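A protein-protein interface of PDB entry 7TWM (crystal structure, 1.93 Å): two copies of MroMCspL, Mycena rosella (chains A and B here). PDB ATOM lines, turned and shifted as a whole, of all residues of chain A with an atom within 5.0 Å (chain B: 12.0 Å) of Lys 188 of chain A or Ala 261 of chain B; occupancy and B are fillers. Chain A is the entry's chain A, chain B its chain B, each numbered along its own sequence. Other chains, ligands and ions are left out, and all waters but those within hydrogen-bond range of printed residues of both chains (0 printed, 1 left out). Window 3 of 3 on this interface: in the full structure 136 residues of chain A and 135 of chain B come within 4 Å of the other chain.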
ATOM      1  N   VAL A 177     -20.858 -29.633  -4.540  1.00  0.00           N
ATOM      2  CA  VAL A 177     -20.950 -29.058  -5.871  1.00  0.00           C
ATOM      3  C   VAL A 177     -19.544 -28.936  -6.461  1.00  0.00           C
ATOM      4  O   VAL A 177     -18.670 -28.310  -5.864  1.00  0.00           O
ATOM      5  CB  VAL A 177     -21.697 -27.710  -5.855  1.00  0.00           C
ATOM      6  CG1 VAL A 177     -21.647 -27.046  -7.226  1.00  0.00           C
ATOM      7  CG2 VAL A 177     -23.141 -27.884  -5.399  1.00  0.00           C
ATOM      8  N   GLY A 178     -19.342 -29.574  -7.625  1.00  0.00           N
ATOM      9  CA  GLY A 178     -18.106 -29.504  -8.393  1.00  0.00           C
ATOM     10  C   GLY A 178     -16.934 -30.290  -7.796  1.00  0.00           C
ATOM     11  O   GLY A 178     -15.805 -30.152  -8.267  1.00  0.00           O
ATOM     12  N   ASN A 186     -17.501 -26.519   0.142  1.00  0.00           N
ATOM     13  CA  ASN A 186     -18.595 -25.677  -0.339  1.00  0.00           C
ATOM     14  C   ASN A 186     -18.078 -24.555  -1.242  1.00  0.00           C
ATOM     15  O   ASN A 186     -18.712 -23.506  -1.370  1.00  0.00           O
ATOM     16  CB  ASN A 186     -19.477 -25.157   0.803  1.00  0.00           C
ATOM     17  CG  ASN A 186     -20.537 -26.158   1.216  1.00  0.00           C
ATOM     18  OD1 ASN A 186     -21.012 -26.131   2.345  1.00  0.00           O
ATOM     19  ND2 ASN A 186     -20.889 -27.062   0.319  1.00  0.00           N
ATOM     20  N   GLY A 187     -16.936 -24.804  -1.894  1.00  0.00           N
ATOM     21  CA  GLY A 187     -16.258 -23.814  -2.723  1.00  0.00           C
ATOM     22  C   GLY A 187     -17.074 -23.377  -3.938  1.00  0.00           C
ATOM     23  O   GLY A 187     -16.832 -22.295  -4.470  1.00  0.00           O
ATOM     24  N   LYS A 188     -18.038 -24.212  -4.369  1.00  0.00           N
ATOM     25  CA  LYS A 188     -18.835 -23.915  -5.553  1.00  0.00           C
ATOM     26  C   LYS A 188     -20.330 -23.902  -5.231  1.00  0.00           C
ATOM     27  O   LYS A 188     -21.146 -23.804  -6.140  1.00  0.00           O
ATOM     28  CB  LYS A 188     -18.530 -24.896  -6.697  1.00  0.00           C
ATOM     29  CG  LYS A 188     -17.092 -24.891  -7.208  1.00  0.00           C
ATOM     30  CD  LYS A 188     -16.703 -23.574  -7.871  1.00  0.00           C
ATOM     31  CE  LYS A 188     -15.211 -23.451  -8.088  1.00  0.00           C
ATOM     32  NZ  LYS A 188     -14.886 -22.284  -8.943  1.00  0.00           N
ATOM     33  N   PHE A 189     -20.684 -23.960  -3.945  1.00  0.00           N
ATOM     34  CA  PHE A 189     -22.083 -23.956  -3.531  1.00  0.00           C
ATOM     35  C   PHE A 189     -22.819 -22.738  -4.092  1.00  0.00           C
ATOM     36  O   PHE A 189     -23.996 -22.828  -4.441  1.00  0.00           O
ATOM     37  CB  PHE A 189     -22.207 -24.019  -2.007  1.00  0.00           C
ATOM     38  CG  PHE A 189     -23.630 -23.897  -1.524  1.00  0.00           C
ATOM     39  CD1 PHE A 189     -24.491 -24.985  -1.583  1.00  0.00           C
ATOM     40  CD2 PHE A 189     -24.120 -22.692  -1.042  1.00  0.00           C
ATOM     41  CE1 PHE A 189     -25.806 -24.874  -1.157  1.00  0.00           C
ATOM     42  CE2 PHE A 189     -25.432 -22.582  -0.610  1.00  0.00           C
ATOM     43  CZ  PHE A 189     -26.280 -23.670  -0.690  1.00  0.00           C
ATOM     44  N   HIS A 190     -22.127 -21.587  -4.145  1.00  0.00           N
ATOM     45  CA  HIS A 190     -22.680 -20.362  -4.702  1.00  0.00           C
ATOM     46  C   HIS A 190     -23.205 -20.548  -6.125  1.00  0.00           C
ATOM     47  O   HIS A 190     -24.090 -19.810  -6.550  1.00  0.00           O
ATOM     48  CB  HIS A 190     -21.671 -19.199  -4.613  1.00  0.00           C
ATOM     49  CG  HIS A 190     -20.507 -19.308  -5.540  1.00  0.00           C
ATOM     50  ND1 HIS A 190     -19.414 -20.115  -5.264  1.00  0.00           N
ATOM     51  CD2 HIS A 190     -20.235 -18.695  -6.716  1.00  0.00           C
ATOM     52  CE1 HIS A 190     -18.521 -19.997  -6.232  1.00  0.00           C
ATOM     53  NE2 HIS A 190     -19.000 -19.130  -7.139  1.00  0.00           N
ATOM     54  N   LEU A 191     -22.671 -21.522  -6.876  1.00  0.00           N
ATOM     55  CA  LEU A 191     -23.159 -21.708  -8.235  1.00  0.00           C
ATOM     56  C   LEU A 191     -24.550 -22.340  -8.216  1.00  0.00           C
ATOM     57  O   LEU A 191     -25.386 -22.023  -9.059  1.00  0.00           O
ATOM     58  CB  LEU A 191     -22.160 -22.537  -9.053  1.00  0.00           C
ATOM     59  CG  LEU A 191     -20.829 -21.848  -9.353  1.00  0.00           C
ATOM     60  CD1 LEU A 191     -19.980 -22.734 -10.251  1.00  0.00           C
ATOM     61  CD2 LEU A 191     -21.049 -20.484 -10.004  1.00  0.00           C
ATOM     62  N   LEU A 192     -24.812 -23.211  -7.236  1.00  0.00           N
ATOM     63  CA  LEU A 192     -26.157 -23.748  -7.075  1.00  0.00           C
ATOM     64  C   LEU A 192     -27.126 -22.641  -6.649  1.00  0.00           C
ATOM     65  O   LEU A 192     -28.273 -22.595  -7.090  1.00  0.00           O
ATOM     66  CB  LEU A 192     -26.135 -24.887  -6.043  1.00  0.00           C
ATOM     67  CG  LEU A 192     -27.498 -25.530  -5.759  1.00  0.00           C
ATOM     68  CD1 LEU A 192     -28.107 -26.130  -7.025  1.00  0.00           C
ATOM     69  CD2 LEU A 192     -27.390 -26.580  -4.656  1.00  0.00           C
ATOM     70  N   ILE B 254     -22.721 -32.261 -21.811  1.00  0.00           N
ATOM     71  CA  ILE B 254     -21.903 -31.655 -20.775  1.00  0.00           C
ATOM     72  C   ILE B 254     -21.340 -30.353 -21.341  1.00  0.00           C
ATOM     73  O   ILE B 254     -20.723 -30.357 -22.405  1.00  0.00           O
ATOM     74  CB  ILE B 254     -20.778 -32.617 -20.335  1.00  0.00           C
ATOM     75  CG1 ILE B 254     -21.303 -33.990 -19.901  1.00  0.00           C
ATOM     76  CG2 ILE B 254     -19.895 -31.983 -19.266  1.00  0.00           C
ATOM     77  CD1 ILE B 254     -22.256 -33.970 -18.721  1.00  0.00           C
ATOM     78  N   ASP B 255     -21.584 -29.242 -20.641  1.00  0.00           N
ATOM     79  CA  ASP B 255     -21.080 -27.948 -21.070  1.00  0.00           C
ATOM     80  C   ASP B 255     -19.661 -27.779 -20.533  1.00  0.00           C
ATOM     81  O   ASP B 255     -19.465 -27.642 -19.325  1.00  0.00           O
ATOM     82  CB  ASP B 255     -22.014 -26.816 -20.638  1.00  0.00           C
ATOM     83  CG  ASP B 255     -21.525 -25.432 -21.036  1.00  0.00           C
ATOM     84  OD1 ASP B 255     -20.427 -25.331 -21.641  1.00  0.00           O
ATOM     85  OD2 ASP B 255     -22.247 -24.466 -20.740  1.00  0.00           O
ATOM     86  N   PRO B 256     -18.624 -27.807 -21.407  1.00  0.00           N
ATOM     87  CA  PRO B 256     -17.237 -27.683 -20.957  1.00  0.00           C
ATOM     88  C   PRO B 256     -16.966 -26.387 -20.192  1.00  0.00           C
ATOM     89  O   PRO B 256     -16.066 -26.346 -19.354  1.00  0.00           O
ATOM     90  CB  PRO B 256     -16.416 -27.752 -22.255  1.00  0.00           C
ATOM     91  CG  PRO B 256     -17.408 -27.412 -23.351  1.00  0.00           C
ATOM     92  CD  PRO B 256     -18.730 -27.968 -22.870  1.00  0.00           C
ATOM     93  N   LYS B 257     -17.766 -25.349 -20.471  1.00  0.00           N
ATOM     94  CA  LYS B 257     -17.643 -24.078 -19.776  1.00  0.00           C
ATOM     95  C   LYS B 257     -18.178 -24.206 -18.353  1.00  0.00           C
ATOM     96  O   LYS B 257     -17.607 -23.621 -17.437  1.00  0.00           O
ATOM     97  CB  LYS B 257     -18.356 -22.949 -20.528  1.00  0.00           C
ATOM     98  CG  LYS B 257     -17.537 -22.297 -21.637  1.00  0.00           C
ATOM     99  CD  LYS B 257     -18.335 -21.325 -22.489  1.00  0.00           C
ATOM    100  CE  LYS B 257     -19.141 -21.995 -23.585  1.00  0.00           C
ATOM    101  NZ  LYS B 257     -18.307 -22.330 -24.766  1.00  0.00           N
ATOM    102  N   ALA B 258     -19.284 -24.950 -18.189  1.00  0.00           N
ATOM    103  CA  ALA B 258     -19.867 -25.175 -16.873  1.00  0.00           C
ATOM    104  C   ALA B 258     -18.927 -26.049 -16.052  1.00  0.00           C
ATOM    105  O   ALA B 258     -18.771 -25.809 -14.858  1.00  0.00           O
ATOM    106  CB  ALA B 258     -21.247 -25.778 -16.972  1.00  0.00           C
ATOM    107  N   VAL B 259     -18.287 -27.030 -16.710  1.00  0.00           N
ATOM    108  CA  VAL B 259     -17.304 -27.888 -16.061  1.00  0.00           C
ATOM    109  C   VAL B 259     -16.170 -27.009 -15.535  1.00  0.00           C
ATOM    110  O   VAL B 259     -15.734 -27.161 -14.397  1.00  0.00           O
ATOM    111  CB  VAL B 259     -16.791 -28.993 -17.008  1.00  0.00           C
ATOM    112  CG1 VAL B 259     -15.589 -29.751 -16.444  1.00  0.00           C
ATOM    113  CG2 VAL B 259     -17.898 -29.978 -17.353  1.00  0.00           C
ATOM    114  N   GLN B 260     -15.714 -26.083 -16.384  1.00  0.00           N
ATOM    115  CA  GLN B 260     -14.662 -25.137 -16.041  1.00  0.00           C
ATOM    116  C   GLN B 260     -15.051 -24.343 -14.789  1.00  0.00           C
ATOM    117  O   GLN B 260     -14.300 -24.317 -13.816  1.00  0.00           O
ATOM    118  CB  GLN B 260     -14.380 -24.230 -17.243  1.00  0.00           C
ATOM    119  CG  GLN B 260     -13.474 -23.046 -16.930  1.00  0.00           C
ATOM    120  CD  GLN B 260     -12.015 -23.413 -17.006  1.00  0.00           C
ATOM    121  OE1 GLN B 260     -11.457 -23.608 -18.087  1.00  0.00           O
ATOM    122  NE2 GLN B 260     -11.377 -23.499 -15.849  1.00  0.00           N
ATOM    123  N   ALA B 261     -16.236 -23.717 -14.821  1.00  0.00           N
ATOM    124  CA  ALA B 261     -16.703 -22.855 -13.745  1.00  0.00           C
ATOM    125  C   ALA B 261     -16.781 -23.628 -12.428  1.00  0.00           C
ATOM    126  O   ALA B 261     -16.558 -23.066 -11.357  1.00  0.00           O
ATOM    127  CB  ALA B 261     -18.038 -22.268 -14.112  1.00  0.00           C
ATOM    128  N   LEU B 262     -17.115 -24.922 -12.516  1.00  0.00           N
ATOM    129  CA  LEU B 262     -17.255 -25.741 -11.324  1.00  0.00           C
ATOM    130  C   LEU B 262     -15.899 -26.181 -10.773  1.00  0.00           C
ATOM    131  O   LEU B 262     -15.841 -26.763  -9.690  1.00  0.00           O
ATOM    132  CB  LEU B 262     -18.146 -26.945 -11.644  1.00  0.00           C
ATOM    133  CG  LEU B 262     -19.640 -26.641 -11.624  1.00  0.00           C
ATOM    134  CD1 LEU B 262     -20.403 -27.633 -12.492  1.00  0.00           C
ATOM    135  CD2 LEU B 262     -20.160 -26.677 -10.199  1.00  0.00           C
ATOM    136  N   GLY B 263     -14.815 -25.908 -11.511  1.00  0.00           N
ATOM    137  CA  GLY B 263     -13.485 -26.287 -11.051  1.00  0.00           C
ATOM    138  C   GLY B 263     -13.179 -27.768 -11.273  1.00  0.00           C
ATOM    139  O   GLY B 263     -12.257 -28.315 -10.668  1.00  0.00           O
ATOM    140  N   LEU B 264     -13.975 -28.416 -12.135  1.00  0.00           N
ATOM    141  CA  LEU B 264     -13.766 -29.813 -12.483  1.00  0.00           C
ATOM    142  C   LEU B 264     -12.727 -29.901 -13.601  1.00  0.00           C
ATOM    143  O   LEU B 264     -12.592 -28.968 -14.394  1.00  0.00           O
ATOM    144  CB  LEU B 264     -15.100 -30.426 -12.919  1.00  0.00           C
ATOM    145  CG  LEU B 264     -16.075 -30.778 -11.794  1.00  0.00           C
ATOM    146  CD1 LEU B 264     -17.494 -30.877 -12.333  1.00  0.00           C
ATOM    147  CD2 LEU B 264     -15.682 -32.072 -11.090  1.00  0.00           C
ATOM    148  N   PRO B 265     -11.965 -31.019 -13.704  1.00  0.00           N
ATOM    149  CA  PRO B 265     -10.973 -31.178 -14.769  1.00  0.00           C
ATOM    150  C   PRO B 265     -11.621 -31.267 -16.149  1.00  0.00           C
ATOM    151  O   PRO B 265     -12.786 -31.641 -16.274  1.00  0.00           O
ATOM    152  CB  PRO B 265     -10.236 -32.475 -14.392  1.00  0.00           C
ATOM    153  CG  PRO B 265     -11.242 -33.242 -13.555  1.00  0.00           C
ATOM    154  CD  PRO B 265     -11.997 -32.173 -12.788  1.00  0.00           C
ATOM    155  N   ALA B 266     -10.847 -30.903 -17.180  1.00  0.00           N
ATOM    156  CA  ALA B 266     -11.326 -30.854 -18.555  1.00  0.00           C
ATOM    157  C   ALA B 266     -11.544 -32.270 -19.086  1.00  0.00           C
ATOM    158  O   ALA B 266     -12.082 -32.442 -20.177  1.00  0.00           O
ATOM    159  CB  ALA B 266     -10.361 -30.077 -19.426  1.00  0.00           C
ATOM    160  N   THR B 267     -11.132 -33.272 -18.297  1.00  0.00           N
ATOM    161  CA  THR B 267     -11.363 -34.677 -18.604  1.00  0.00           C
ATOM    162  C   THR B 267     -12.839 -35.047 -18.422  1.00  0.00           C
ATOM    163  O   THR B 267     -13.296 -36.052 -18.968  1.00  0.00           O
ATOM    164  CB  THR B 267     -10.393 -35.601 -17.848  1.00  0.00           C
ATOM    165  OG1 THR B 267     -10.488 -35.367 -16.442  1.00  0.00           O
ATOM    166  CG2 THR B 267      -8.952 -35.443 -18.288  1.00  0.00           C
ATOM    167  N   VAL B 268     -13.587 -34.228 -17.668  1.00  0.00           N
ATOM    168  CA  VAL B 268     -15.012 -34.455 -17.473  1.00  0.00           C
ATOM    169  C   VAL B 268     -15.749 -34.090 -18.762  1.00  0.00           C
ATOM    170  O   VAL B 268     -16.084 -32.928 -18.995  1.00  0.00           O
ATOM    171  CB  VAL B 268     -15.570 -33.700 -16.245  1.00  0.00           C
ATOM    172  CG1 VAL B 268     -17.087 -33.819 -16.144  1.00  0.00           C
ATOM    173  CG2 VAL B 268     -14.918 -34.164 -14.949  1.00  0.00           C
ATOM    174  N   VAL B 401     -20.323 -37.008 -11.264  1.00  0.00           N
ATOM    175  CA  VAL B 401     -20.819 -36.719 -12.598  1.00  0.00           C
ATOM    176  C   VAL B 401     -19.790 -37.186 -13.631  1.00  0.00           C
ATOM    177  O   VAL B 401     -20.166 -37.688 -14.690  1.00  0.00           O
ATOM    178  CB  VAL B 401     -21.217 -35.237 -12.764  1.00  0.00           C
ATOM    179  CG1 VAL B 401     -22.134 -35.030 -13.961  1.00  0.00           C
ATOM    180  CG2 VAL B 401     -21.900 -34.711 -11.511  1.00  0.00           C
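Of chain B, only Leu 262 comes within 4 Å of Val 177 of chain A. No residue of chain B comes within 4 Å of Asn 186 of chain A. No residue of chain B comes within 4 Å of Gly 187 of chain A. Of chain B, only Ala 261 and Leu 262 come within 4 Å of Lys 188 of chain A. No residue of chain B comes within 4 Å of Phe 189 of chain A. No residue of chain B comes within 4 Å of His 190 of chain A. No residue of chain B comes within 4 Å of Leu 192 of chain A. Asp 255 of chain B touches none of the printed residues of chain A. Of chain A, only Lys 188 and Leu 191 come within 4 Å of Ala 261 of chain B. Printed residues of chain A within 4 Å of Leu 262 of chain B: Val 177 (3.3 Å), Gly 178 (3.7 Å), Lys 188 (3.4 Å) and Leu 191 (3.9 Å). Of the printed residues of chain A, Leu 264 of chain B touches Gly 178.
The backbone carbonyl oxygen (O) of Ala 261 of chain B sits at hydrogen-bond distance from the side-chain amino group (NZ) of Lys 188 of chain A (3.0 Å).
The backbone NH (N) of Leu 264 of chain B sits at hydrogen-bond distance from the backbone carbonyl oxygen (O) of Val 259 of chain B, 3.1 Å away.
No position is printed for both chains. Of the 7 pairs that touch across the chains among the printed residues, none has its exchanged pair printed and touching as well.
Of the 9 printed residues of chain A, 4 touch a printed residue of chain B. Hydrophobic or aromatic side chains of chain A that line the printed part of chain B: Val 177 and Leu 191. Hydrophobic or aromatic side chains of chain B that line the printed part of chain A: Leu 262 and Leu 264. Along chain B the printed residues that touch a printed residue of chain A span positions 261 to 264. Among the printed residues, 7 pairs touch across the chains.
Among the printed residues, pairs that only touch across the chains: Val 177 of chain A with Leu 262 of chain B, Lys 188 of chain A with Leu 262 of chain B, Gly 178 of chain A with Leu 264 of chain B, Leu 191 of chain A with Ala 261 of chain B, Gly 178 of chain A with Leu 262 of chain B and Leu 191 of chain A with Leu 262 of chain B.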
